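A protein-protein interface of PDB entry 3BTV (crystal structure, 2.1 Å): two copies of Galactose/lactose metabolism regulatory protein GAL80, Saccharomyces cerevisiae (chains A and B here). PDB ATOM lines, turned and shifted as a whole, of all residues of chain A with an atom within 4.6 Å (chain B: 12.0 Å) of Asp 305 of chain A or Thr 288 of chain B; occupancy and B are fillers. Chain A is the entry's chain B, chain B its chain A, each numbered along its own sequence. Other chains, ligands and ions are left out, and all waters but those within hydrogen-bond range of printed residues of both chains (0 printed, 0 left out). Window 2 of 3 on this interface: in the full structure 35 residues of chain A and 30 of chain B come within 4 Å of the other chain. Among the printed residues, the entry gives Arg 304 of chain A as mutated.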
ATOM      1  N   ILE A 299      18.434 -16.350  17.994  1.00  0.00           N
ATOM      2  CA  ILE A 299      19.098 -16.458  19.291  1.00  0.00           C
ATOM      3  C   ILE A 299      18.298 -17.408  20.182  1.00  0.00           C
ATOM      4  O   ILE A 299      17.144 -17.161  20.469  1.00  0.00           O
ATOM      5  CB  ILE A 299      19.250 -15.079  19.928  1.00  0.00           C
ATOM      6  CG1 ILE A 299      20.044 -14.180  18.976  1.00  0.00           C
ATOM      7  CG2 ILE A 299      19.935 -15.174  21.291  1.00  0.00           C
ATOM      8  CD1 ILE A 299      20.310 -12.800  19.483  1.00  0.00           C
ATOM      9  N   HIS A 300      18.890 -18.536  20.557  1.00  0.00           N
ATOM     10  CA  HIS A 300      18.157 -19.533  21.350  1.00  0.00           C
ATOM     11  C   HIS A 300      18.537 -19.398  22.817  1.00  0.00           C
ATOM     12  O   HIS A 300      19.712 -19.584  23.190  1.00  0.00           O
ATOM     13  CB  HIS A 300      18.481 -20.936  20.840  1.00  0.00           C
ATOM     14  CG  HIS A 300      18.343 -21.073  19.358  1.00  0.00           C
ATOM     15  ND1 HIS A 300      17.115 -21.172  18.737  1.00  0.00           N
ATOM     16  CD2 HIS A 300      19.275 -21.131  18.369  1.00  0.00           C
ATOM     17  CE1 HIS A 300      17.293 -21.286  17.429  1.00  0.00           C
ATOM     18  NE2 HIS A 300      18.594 -21.260  17.181  1.00  0.00           N
ATOM     19  N   GLY A 301      17.557 -19.038  23.638  1.00  0.00           N
ATOM     20  CA  GLY A 301      17.755 -18.844  25.070  1.00  0.00           C
ATOM     21  C   GLY A 301      17.255 -20.033  25.864  1.00  0.00           C
ATOM     22  O   GLY A 301      16.570 -20.885  25.330  1.00  0.00           O
ATOM     23  N   ARG A 304      13.404 -18.446  26.367  1.00  0.00           N
ATOM     24  CA  ARG A 304      12.680 -18.045  25.171  1.00  0.00           C
ATOM     25  C   ARG A 304      13.637 -17.979  24.008  1.00  0.00           C
ATOM     26  O   ARG A 304      14.856 -17.890  24.205  1.00  0.00           O
ATOM     27  CB  ARG A 304      12.058 -16.655  25.338  1.00  0.00           C
ATOM     28  CG  ARG A 304      10.928 -16.551  26.353  1.00  0.00           C
ATOM     29  CD  ARG A 304      10.274 -15.160  26.256  1.00  0.00           C
ATOM     30  NE  ARG A 304       9.181 -14.998  27.204  1.00  0.00           N
ATOM     31  CZ  ARG A 304       9.340 -14.801  28.511  1.00  0.00           C
ATOM     32  NH1 ARG A 304      10.557 -14.736  29.039  1.00  0.00           N
ATOM     33  NH2 ARG A 304       8.276 -14.665  29.295  1.00  0.00           N
ATOM     34  N   ASP A 305      13.088 -18.030  22.798  1.00  0.00           N
ATOM     35  CA  ASP A 305      13.878 -17.769  21.601  1.00  0.00           C
ATOM     36  C   ASP A 305      13.539 -16.392  21.069  1.00  0.00           C
ATOM     37  O   ASP A 305      12.400 -15.918  21.198  1.00  0.00           O
ATOM     38  CB  ASP A 305      13.590 -18.796  20.512  1.00  0.00           C
ATOM     39  CG  ASP A 305      14.180 -20.165  20.831  1.00  0.00           C
ATOM     40  OD1 ASP A 305      14.935 -20.284  21.827  1.00  0.00           O
ATOM     41  OD2 ASP A 305      13.884 -21.116  20.081  1.00  0.00           O
ATOM     42  N   LEU A 306      14.531 -15.767  20.452  1.00  0.00           N
ATOM     43  CA  LEU A 306      14.382 -14.448  19.855  1.00  0.00           C
ATOM     44  C   LEU A 306      14.857 -14.576  18.415  1.00  0.00           C
ATOM     45  O   LEU A 306      15.872 -15.200  18.158  1.00  0.00           O
ATOM     46  CB  LEU A 306      15.273 -13.474  20.622  1.00  0.00           C
ATOM     47  CG  LEU A 306      15.323 -11.996  20.307  1.00  0.00           C
ATOM     48  CD1 LEU A 306      15.835 -11.268  21.543  1.00  0.00           C
ATOM     49  CD2 LEU A 306      16.268 -11.801  19.157  1.00  0.00           C
ATOM     50  N   LYS A 307      14.125 -13.989  17.492  1.00  0.00           N
ATOM     51  CA  LYS A 307      14.509 -13.984  16.086  1.00  0.00           C
ATOM     52  C   LYS A 307      14.347 -12.591  15.458  1.00  0.00           C
ATOM     53  O   LYS A 307      13.296 -11.935  15.582  1.00  0.00           O
ATOM     54  CB  LYS A 307      13.682 -15.008  15.308  1.00  0.00           C
ATOM     55  CG  LYS A 307      13.951 -14.985  13.801  1.00  0.00           C
ATOM     56  CD  LYS A 307      12.723 -15.470  13.015  1.00  0.00           C
ATOM     57  CE  LYS A 307      12.562 -16.982  13.105  1.00  0.00           C
ATOM     58  NZ  LYS A 307      13.768 -17.687  12.548  1.00  0.00           N
ATOM     59  N   VAL A 321      10.862 -11.126  16.666  1.00  0.00           N
ATOM     60  CA  VAL A 321       9.912 -12.099  17.186  1.00  0.00           C
ATOM     61  C   VAL A 321      10.455 -12.804  18.429  1.00  0.00           C
ATOM     62  O   VAL A 321      11.607 -13.233  18.455  1.00  0.00           O
ATOM     63  CB  VAL A 321       9.590 -13.173  16.130  1.00  0.00           C
ATOM     64  CG1 VAL A 321       8.439 -14.037  16.606  1.00  0.00           C
ATOM     65  CG2 VAL A 321       9.227 -12.524  14.783  1.00  0.00           C
ATOM     66  N   LEU A 322       9.605 -12.946  19.439  1.00  0.00           N
ATOM     67  CA  LEU A 322       9.932 -13.677  20.654  1.00  0.00           C
ATOM     68  C   LEU A 322       8.961 -14.814  20.836  1.00  0.00           C
ATOM     69  O   LEU A 322       7.743 -14.627  20.699  1.00  0.00           O
ATOM     70  CB  LEU A 322       9.814 -12.768  21.873  1.00  0.00           C
ATOM     71  CG  LEU A 322      10.985 -11.855  22.187  1.00  0.00           C
ATOM     72  CD1 LEU A 322      10.510 -10.833  23.189  1.00  0.00           C
ATOM     73  CD2 LEU A 322      12.140 -12.683  22.745  1.00  0.00           C
ATOM     74  N   TYR A 323       9.500 -15.971  21.209  1.00  0.00           N
ATOM     75  CA  TYR A 323       8.722 -17.204  21.308  1.00  0.00           C
ATOM     76  C   TYR A 323       8.962 -17.865  22.639  1.00  0.00           C
ATOM     77  O   TYR A 323      10.118 -18.068  23.043  1.00  0.00           O
ATOM     78  CB  TYR A 323       9.163 -18.234  20.278  1.00  0.00           C
ATOM     79  CG  TYR A 323       9.306 -17.791  18.853  1.00  0.00           C
ATOM     80  CD1 TYR A 323       8.312 -18.072  17.926  1.00  0.00           C
ATOM     81  CD2 TYR A 323      10.467 -17.170  18.409  1.00  0.00           C
ATOM     82  CE1 TYR A 323       8.446 -17.714  16.605  1.00  0.00           C
ATOM     83  CE2 TYR A 323      10.620 -16.821  17.083  1.00  0.00           C
ATOM     84  CZ  TYR A 323       9.600 -17.091  16.186  1.00  0.00           C
ATOM     85  OH  TYR A 323       9.716 -16.726  14.864  1.00  0.00           O
ATOM     86  N   TYR A 324       7.871 -18.251  23.286  1.00  0.00           N
ATOM     87  CA  TYR A 324       7.901 -18.979  24.543  1.00  0.00           C
ATOM     88  C   TYR A 324       7.058 -20.243  24.418  1.00  0.00           C
ATOM     89  O   TYR A 324       6.072 -20.266  23.675  1.00  0.00           O
ATOM     90  CB  TYR A 324       7.329 -18.116  25.672  1.00  0.00           C
ATOM     91  CG  TYR A 324       6.955 -18.935  26.887  1.00  0.00           C
ATOM     92  CD1 TYR A 324       7.908 -19.289  27.835  1.00  0.00           C
ATOM     93  CD2 TYR A 324       5.655 -19.383  27.074  1.00  0.00           C
ATOM     94  CE1 TYR A 324       7.569 -20.052  28.942  1.00  0.00           C
ATOM     95  CE2 TYR A 324       5.308 -20.146  28.174  1.00  0.00           C
ATOM     96  CZ  TYR A 324       6.265 -20.477  29.105  1.00  0.00           C
ATOM     97  OH  TYR A 324       5.912 -21.236  30.199  1.00  0.00           O
ATOM     98  N   SER A 325       7.423 -21.288  25.157  1.00  0.00           N
ATOM     99  CA  SER A 325       6.621 -22.512  25.167  1.00  0.00           C
ATOM    100  C   SER A 325       6.480 -23.159  26.545  1.00  0.00           C
ATOM    101  O   SER A 325       7.350 -23.018  27.403  1.00  0.00           O
ATOM    102  CB  SER A 325       7.180 -23.522  24.168  1.00  0.00           C
ATOM    103  OG  SER A 325       8.503 -23.897  24.507  1.00  0.00           O
ATOM    104  N   ALA B 182      20.709 -27.675  10.081  1.00  0.00           N
ATOM    105  CA  ALA B 182      20.464 -27.369  11.475  1.00  0.00           C
ATOM    106  C   ALA B 182      19.749 -28.575  12.038  1.00  0.00           C
ATOM    107  O   ALA B 182      18.781 -29.052  11.446  1.00  0.00           O
ATOM    108  CB  ALA B 182      19.619 -26.120  11.579  1.00  0.00           C
ATOM    109  N   GLY B 183      20.265 -29.111  13.136  1.00  0.00           N
ATOM    110  CA  GLY B 183      19.679 -30.287  13.742  1.00  0.00           C
ATOM    111  C   GLY B 183      19.610 -30.247  15.259  1.00  0.00           C
ATOM    112  O   GLY B 183      20.141 -29.340  15.903  1.00  0.00           O
ATOM    113  N   ASN B 184      18.871 -31.193  15.838  1.00  0.00           N
ATOM    114  CA  ASN B 184      18.846 -31.395  17.291  1.00  0.00           C
ATOM    115  C   ASN B 184      19.203 -32.854  17.601  1.00  0.00           C
ATOM    116  O   ASN B 184      18.843 -33.756  16.849  1.00  0.00           O
ATOM    117  CB  ASN B 184      17.467 -31.105  17.906  1.00  0.00           C
ATOM    118  CG  ASN B 184      16.860 -29.773  17.465  1.00  0.00           C
ATOM    119  OD1 ASN B 184      17.441 -28.701  17.650  1.00  0.00           O
ATOM    120  ND2 ASN B 184      15.645 -29.842  16.930  1.00  0.00           N
ATOM    121  N   GLY B 185      19.887 -33.084  18.714  1.00  0.00           N
ATOM    122  CA  GLY B 185      20.223 -34.433  19.163  1.00  0.00           C
ATOM    123  C   GLY B 185      19.284 -35.107  20.167  1.00  0.00           C
ATOM    124  O   GLY B 185      19.582 -36.193  20.684  1.00  0.00           O
ATOM    125  N   GLY B 186      18.155 -34.477  20.468  1.00  0.00           N
ATOM    126  CA  GLY B 186      17.200 -35.075  21.390  1.00  0.00           C
ATOM    127  C   GLY B 186      17.498 -34.993  22.876  1.00  0.00           C
ATOM    128  O   GLY B 186      16.866 -34.209  23.591  1.00  0.00           O
ATOM    129  N   TRP B 187      18.425 -35.802  23.380  1.00  0.00           N
ATOM    130  CA  TRP B 187      18.540 -35.862  24.854  1.00  0.00           C
ATOM    131  C   TRP B 187      19.840 -35.337  25.456  1.00  0.00           C
ATOM    132  O   TRP B 187      20.214 -35.672  26.583  1.00  0.00           O
ATOM    133  CB  TRP B 187      18.155 -37.241  25.403  1.00  0.00           C
ATOM    134  CG  TRP B 187      16.673 -37.532  25.234  1.00  0.00           C
ATOM    135  CD1 TRP B 187      16.118 -38.558  24.528  1.00  0.00           C
ATOM    136  CD2 TRP B 187      15.570 -36.763  25.755  1.00  0.00           C
ATOM    137  NE1 TRP B 187      14.746 -38.487  24.585  1.00  0.00           N
ATOM    138  CE2 TRP B 187      14.384 -37.395  25.330  1.00  0.00           C
ATOM    139  CE3 TRP B 187      15.474 -35.605  26.540  1.00  0.00           C
ATOM    140  CZ2 TRP B 187      13.112 -36.911  25.663  1.00  0.00           C
ATOM    141  CZ3 TRP B 187      14.210 -35.122  26.872  1.00  0.00           C
ATOM    142  CH2 TRP B 187      13.045 -35.778  26.435  1.00  0.00           C
ATOM    143  N   GLY B 189      20.529 -32.010  25.818  1.00  0.00           N
ATOM    144  CA  GLY B 189      20.327 -30.644  26.272  1.00  0.00           C
ATOM    145  C   GLY B 189      20.328 -30.564  27.796  1.00  0.00           C
ATOM    146  O   GLY B 189      21.065 -31.285  28.490  1.00  0.00           O
ATOM    147  N   TYR B 190      19.491 -29.683  28.332  1.00  0.00           N
ATOM    148  CA  TYR B 190      19.510 -29.400  29.774  1.00  0.00           C
ATOM    149  C   TYR B 190      18.876 -30.513  30.608  1.00  0.00           C
ATOM    150  O   TYR B 190      19.111 -30.615  31.814  1.00  0.00           O
ATOM    151  CB  TYR B 190      18.842 -28.043  30.061  1.00  0.00           C
ATOM    152  CG  TYR B 190      19.620 -26.882  29.477  1.00  0.00           C
ATOM    153  CD1 TYR B 190      19.252 -26.325  28.256  1.00  0.00           C
ATOM    154  CD2 TYR B 190      20.752 -26.374  30.121  1.00  0.00           C
ATOM    155  CE1 TYR B 190      19.959 -25.270  27.713  1.00  0.00           C
ATOM    156  CE2 TYR B 190      21.473 -25.319  29.578  1.00  0.00           C
ATOM    157  CZ  TYR B 190      21.069 -24.775  28.368  1.00  0.00           C
ATOM    158  OH  TYR B 190      21.765 -23.722  27.803  1.00  0.00           O
ATOM    159  N   GLU B 191      18.097 -31.363  29.954  1.00  0.00           N
ATOM    160  CA  GLU B 191      17.330 -32.376  30.666  1.00  0.00           C
ATOM    161  C   GLU B 191      17.619 -33.820  30.238  1.00  0.00           C
ATOM    162  O   GLU B 191      17.941 -34.085  29.075  1.00  0.00           O
ATOM    163  CB  GLU B 191      15.842 -32.043  30.542  1.00  0.00           C
ATOM    164  CG  GLU B 191      15.549 -30.677  31.114  1.00  0.00           C
ATOM    165  CD  GLU B 191      14.076 -30.314  31.054  1.00  0.00           C
ATOM    166  OE1 GLU B 191      13.382 -30.835  30.157  1.00  0.00           O
ATOM    167  OE2 GLU B 191      13.626 -29.512  31.904  1.00  0.00           O
ATOM    168  N   ARG B 252      10.948 -31.655  36.221  1.00  0.00           N
ATOM    169  CA  ARG B 252      12.258 -31.893  36.835  1.00  0.00           C
ATOM    170  C   ARG B 252      12.143 -32.577  38.201  1.00  0.00           C
ATOM    171  O   ARG B 252      11.182 -32.366  38.935  1.00  0.00           O
ATOM    172  CB  ARG B 252      13.036 -30.579  36.947  1.00  0.00           C
ATOM    173  CG  ARG B 252      13.270 -29.917  35.597  1.00  0.00           C
ATOM    174  CD  ARG B 252      14.344 -28.839  35.624  1.00  0.00           C
ATOM    175  NE  ARG B 252      14.608 -28.339  34.273  1.00  0.00           N
ATOM    176  CZ  ARG B 252      15.436 -27.339  33.989  1.00  0.00           C
ATOM    177  NH1 ARG B 252      16.109 -26.728  34.953  1.00  0.00           N
ATOM    178  NH2 ARG B 252      15.600 -26.954  32.731  1.00  0.00           N
ATOM    179  N   HIS B 264      26.661 -29.454  21.975  1.00  0.00           N
ATOM    180  CA  HIS B 264      26.565 -28.677  20.741  1.00  0.00           C
ATOM    181  C   HIS B 264      27.674 -28.988  19.749  1.00  0.00           C
ATOM    182  O   HIS B 264      28.801 -29.270  20.131  1.00  0.00           O
ATOM    183  CB  HIS B 264      26.535 -27.174  21.035  1.00  0.00           C
ATOM    184  CG  HIS B 264      25.778 -26.373  20.019  1.00  0.00           C
ATOM    185  ND1 HIS B 264      26.371 -25.849  18.886  1.00  0.00           N
ATOM    186  CD2 HIS B 264      24.471 -26.009  19.963  1.00  0.00           C
ATOM    187  CE1 HIS B 264      25.462 -25.195  18.179  1.00  0.00           C
ATOM    188  NE2 HIS B 264      24.306 -25.264  18.818  1.00  0.00           N
ATOM    189  N   SER B 281      24.915 -26.655  12.279  1.00  0.00           N
ATOM    190  CA  SER B 281      24.805 -26.405  13.715  1.00  0.00           C
ATOM    191  C   SER B 281      23.864 -27.447  14.324  1.00  0.00           C
ATOM    192  O   SER B 281      22.700 -27.550  13.935  1.00  0.00           O
ATOM    193  CB  SER B 281      24.243 -25.000  13.962  1.00  0.00           C
ATOM    194  OG  SER B 281      24.162 -24.709  15.346  1.00  0.00           O
ATOM    195  N   LYS B 283      22.267 -28.767  17.931  1.00  0.00           N
ATOM    196  CA  LYS B 283      22.005 -28.525  19.353  1.00  0.00           C
ATOM    197  C   LYS B 283      21.811 -29.867  20.053  1.00  0.00           C
ATOM    198  O   LYS B 283      21.176 -30.776  19.516  1.00  0.00           O
ATOM    199  CB  LYS B 283      20.737 -27.658  19.510  1.00  0.00           C
ATOM    200  CG  LYS B 283      20.787 -26.360  18.720  1.00  0.00           C
ATOM    201  CD  LYS B 283      19.413 -25.722  18.570  1.00  0.00           C
ATOM    202  CE  LYS B 283      19.102 -24.776  19.722  1.00  0.00           C
ATOM    203  NZ  LYS B 283      19.108 -25.458  21.047  1.00  0.00           N
ATOM    204  N   GLY B 284      22.334 -29.995  21.262  1.00  0.00           N
ATOM    205  CA  GLY B 284      22.220 -31.250  21.997  1.00  0.00           C
ATOM    206  C   GLY B 284      20.814 -31.738  22.294  1.00  0.00           C
ATOM    207  O   GLY B 284      20.493 -32.924  22.150  1.00  0.00           O
ATOM    208  N   GLY B 285      19.997 -30.725  22.539  1.00  0.00           N
ATOM    209  CA  GLY B 285      18.834 -30.633  23.376  1.00  0.00           C
ATOM    210  C   GLY B 285      17.529 -30.526  22.654  1.00  0.00           C
ATOM    211  O   GLY B 285      17.211 -31.410  21.886  1.00  0.00           O
ATOM    212  N   LYS B 286      16.741 -29.503  22.964  1.00  0.00           N
ATOM    213  CA  LYS B 286      15.363 -29.435  22.480  1.00  0.00           C
ATOM    214  C   LYS B 286      14.986 -27.995  22.142  1.00  0.00           C
ATOM    215  O   LYS B 286      15.548 -27.051  22.698  1.00  0.00           O
ATOM    216  CB  LYS B 286      14.410 -30.002  23.541  1.00  0.00           C
ATOM    217  CG  LYS B 286      13.383 -30.995  23.009  1.00  0.00           C
ATOM    218  CD  LYS B 286      14.006 -31.938  21.974  1.00  0.00           C
ATOM    219  CE  LYS B 286      13.360 -33.319  22.020  1.00  0.00           C
ATOM    220  NZ  LYS B 286      13.644 -34.114  20.787  1.00  0.00           N
ATOM    221  N   PRO B 287      14.034 -27.818  21.219  1.00  0.00           N
ATOM    222  CA  PRO B 287      13.702 -26.473  20.754  1.00  0.00           C
ATOM    223  C   PRO B 287      12.380 -25.919  21.278  1.00  0.00           C
ATOM    224  O   PRO B 287      11.408 -26.657  21.431  1.00  0.00           O
ATOM    225  CB  PRO B 287      13.635 -26.677  19.247  1.00  0.00           C
ATOM    226  CG  PRO B 287      13.029 -28.070  19.114  1.00  0.00           C
ATOM    227  CD  PRO B 287      13.429 -28.849  20.358  1.00  0.00           C
ATOM    228  N   THR B 288      12.378 -24.618  21.564  1.00  0.00           N
ATOM    229  CA  THR B 288      11.175 -23.845  21.869  1.00  0.00           C
ATOM    230  C   THR B 288      10.865 -23.167  20.546  1.00  0.00           C
ATOM    231  O   THR B 288      10.934 -21.941  20.437  1.00  0.00           O
ATOM    232  CB  THR B 288      11.505 -22.749  22.915  1.00  0.00           C
ATOM    233  OG1 THR B 288      12.100 -23.343  24.076  1.00  0.00           O
ATOM    234  CG2 THR B 288      10.261 -21.978  23.320  1.00  0.00           C
ATOM    235  N   THR B 292       9.423 -26.220  16.661  1.00  0.00           N
ATOM    236  CA  THR B 292      10.175 -26.038  15.438  1.00  0.00           C
ATOM    237  C   THR B 292      10.242 -27.288  14.576  1.00  0.00           C
ATOM    238  O   THR B 292       9.455 -28.218  14.739  1.00  0.00           O
ATOM    239  CB  THR B 292      11.626 -25.783  15.873  1.00  0.00           C
ATOM    240  OG1 THR B 292      11.791 -26.292  17.203  1.00  0.00           O
ATOM    241  CG2 THR B 292      11.942 -24.311  15.890  1.00  0.00           C
ATOM    242  N   LYS B 293      11.206 -27.292  13.660  1.00  0.00           N
ATOM    243  CA  LYS B 293      11.580 -28.494  12.923  1.00  0.00           C
ATOM    244  C   LYS B 293      12.791 -29.127  13.608  1.00  0.00           C
ATOM    245  O   LYS B 293      13.688 -28.422  14.068  1.00  0.00           O
ATOM    246  CB  LYS B 293      11.906 -28.155  11.466  1.00  0.00           C
ATOM    247  CG  LYS B 293      10.675 -27.926  10.601  1.00  0.00           C
ATOM    248  CD  LYS B 293       9.750 -29.136  10.684  1.00  0.00           C
ATOM    249  CE  LYS B 293       8.635 -29.076   9.656  1.00  0.00           C
ATOM    250  NZ  LYS B 293       7.972 -30.402   9.506  1.00  0.00           N
ATOM    251  N   ASN B 294      12.799 -30.453  13.696  1.00  0.00           N
ATOM    252  CA  ASN B 294      13.845 -31.197  14.398  1.00  0.00           C
ATOM    253  C   ASN B 294      15.161 -31.235  13.596  1.00  0.00           C
ATOM    254  O   ASN B 294      16.262 -31.288  14.152  1.00  0.00           O
ATOM    255  CB  ASN B 294      13.347 -32.619  14.631  1.00  0.00           C
ATOM    256  CG  ASN B 294      14.246 -33.409  15.529  1.00  0.00           C
ATOM    257  OD1 ASN B 294      14.456 -33.054  16.691  1.00  0.00           O
ATOM    258  ND2 ASN B 294      14.770 -34.511  15.008  1.00  0.00           N
ATOM    259  N   LEU B 295      15.020 -31.227  12.276  1.00  0.00           N
ATOM    260  CA  LEU B 295      16.141 -31.300  11.348  1.00  0.00           C
ATOM    261  C   LEU B 295      15.763 -30.531  10.085  1.00  0.00           C
ATOM    262  O   LEU B 295      14.660 -30.701   9.570  1.00  0.00           O
ATOM    263  CB  LEU B 295      16.421 -32.765  11.013  1.00  0.00           C
ATOM    264  CG  LEU B 295      17.502 -33.115   9.985  1.00  0.00           C
ATOM    265  CD1 LEU B 295      17.013 -32.896   8.576  1.00  0.00           C
ATOM    266  CD2 LEU B 295      18.785 -32.316  10.249  1.00  0.00           C
ATOM    267  N   ASP B 311      11.239 -33.869  12.215  1.00  0.00           N
ATOM    268  CA  ASP B 311      10.086 -34.359  12.947  1.00  0.00           C
ATOM    269  C   ASP B 311       9.622 -35.203  11.788  1.00  0.00           C
ATOM    270  O   ASP B 311       8.474 -35.631  11.672  1.00  0.00           O
ATOM    271  CB  ASP B 311       9.115 -33.225  13.256  1.00  0.00           C
ATOM    272  CG  ASP B 311       9.726 -32.167  14.157  1.00  0.00           C
ATOM    273  OD1 ASP B 311       9.520 -30.962  13.897  1.00  0.00           O
ATOM    274  OD2 ASP B 311      10.421 -32.543  15.125  1.00  0.00           O
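OD2 of Asp 305 of chain A lies close to O of Thr 288 of chain B.
The backbone NH (N) of Gly 185 of chain B lies within hydrogen-bond range of the backbone carbonyl oxygen (O) of Lys 283 of chain B, at 2.8 Å. The backbone carbonyl oxygen (O) of Gly 183 of chain B lies within hydrogen-bond range of the backbone NH (N) of Lys 283 of chain B (3.0 Å). The backbone NH of Gly 301 of chain A is in hydrogen-bond range of the side-chain carboxylate of Asp 305 of chain A (3.4 Å). N of Tyr 323 of chain A lies within hydrogen-bond range of O of Asp 305 of chain A (2.9 Å). A ring nitrogen (ND1) of His 300 of chain A sits at hydrogen-bond distance from the side-chain carboxylate (OD2) of Asp 305 of chain A.
Among the printed residues, merely in contact across the chains: His 300 of chain A with Lys 283 of chain B, Tyr 323 of chain A with Thr 288 of chain B, Tyr 324 of chain A with Thr 288 of chain B and Ser 325 of chain A with Thr 288 of chain B.
No residue of chain B comes within 4 Å of Ile 299 of chain A. His 300 of chain A touches one residue of chain B. No residue of chain B comes within 4 Å of Gly 301 of chain A. Of the printed residues of chain B, Asp 305 of chain A touches Thr 288. No residue of chain B comes within 4 Å of Val 321 of chain A. Printed residues of chain B within 4 Å of Tyr 323 of chain A: Thr 288. Of the printed residues of chain B, Tyr 324 of chain A touches Thr 288 (3.8 Å). Ser 325 of chain A touches just one residue of chain B: Thr 288 (2.9 Å). Asn 184 of chain B touches none of the printed residues of chain A. Of the printed residues of chain A, Lys 283 of chain B touches His 300. Of chain A, only Asp 305 (3.1 Å), Tyr 323 (3.9 Å), Tyr 324 (3.8 Å) and Ser 325 (2.9 Å) come within 4 Å of Thr 288 of chain B. Leu 295 of chain B touches none of the printed residues of chain A. The nearest residue of chain B that does not touch Asp 305 of chain A is Pro 287 of chain B (5.2 Å). The nearest printed residue of chain A that does not touch Thr 288 of chain B is Arg 304 of chain A (5.0 Å). The nearest printed residue of chain B that does not touch Tyr 324 of chain A is Pro 287 of chain B (8.3 Å).
Printed residues of chain A that touch a printed residue of chain B: His 300, Asp 305, Tyr 323, Tyr 324 and Ser 325. Hydrophobic or aromatic side chains of chain A that line the printed part of chain B: His 300. Among the printed residues, 5 pairs touch across the chains. Among the printed residues, no Asp or Glu carboxylate lies within 4 Å of a Lys or Arg side-chain nitrogen of the other chain.
No position is printed for both chains. Of the 5 pairs that touch across the chains among the printed residues, none has its exchanged pair printed and touching as well.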
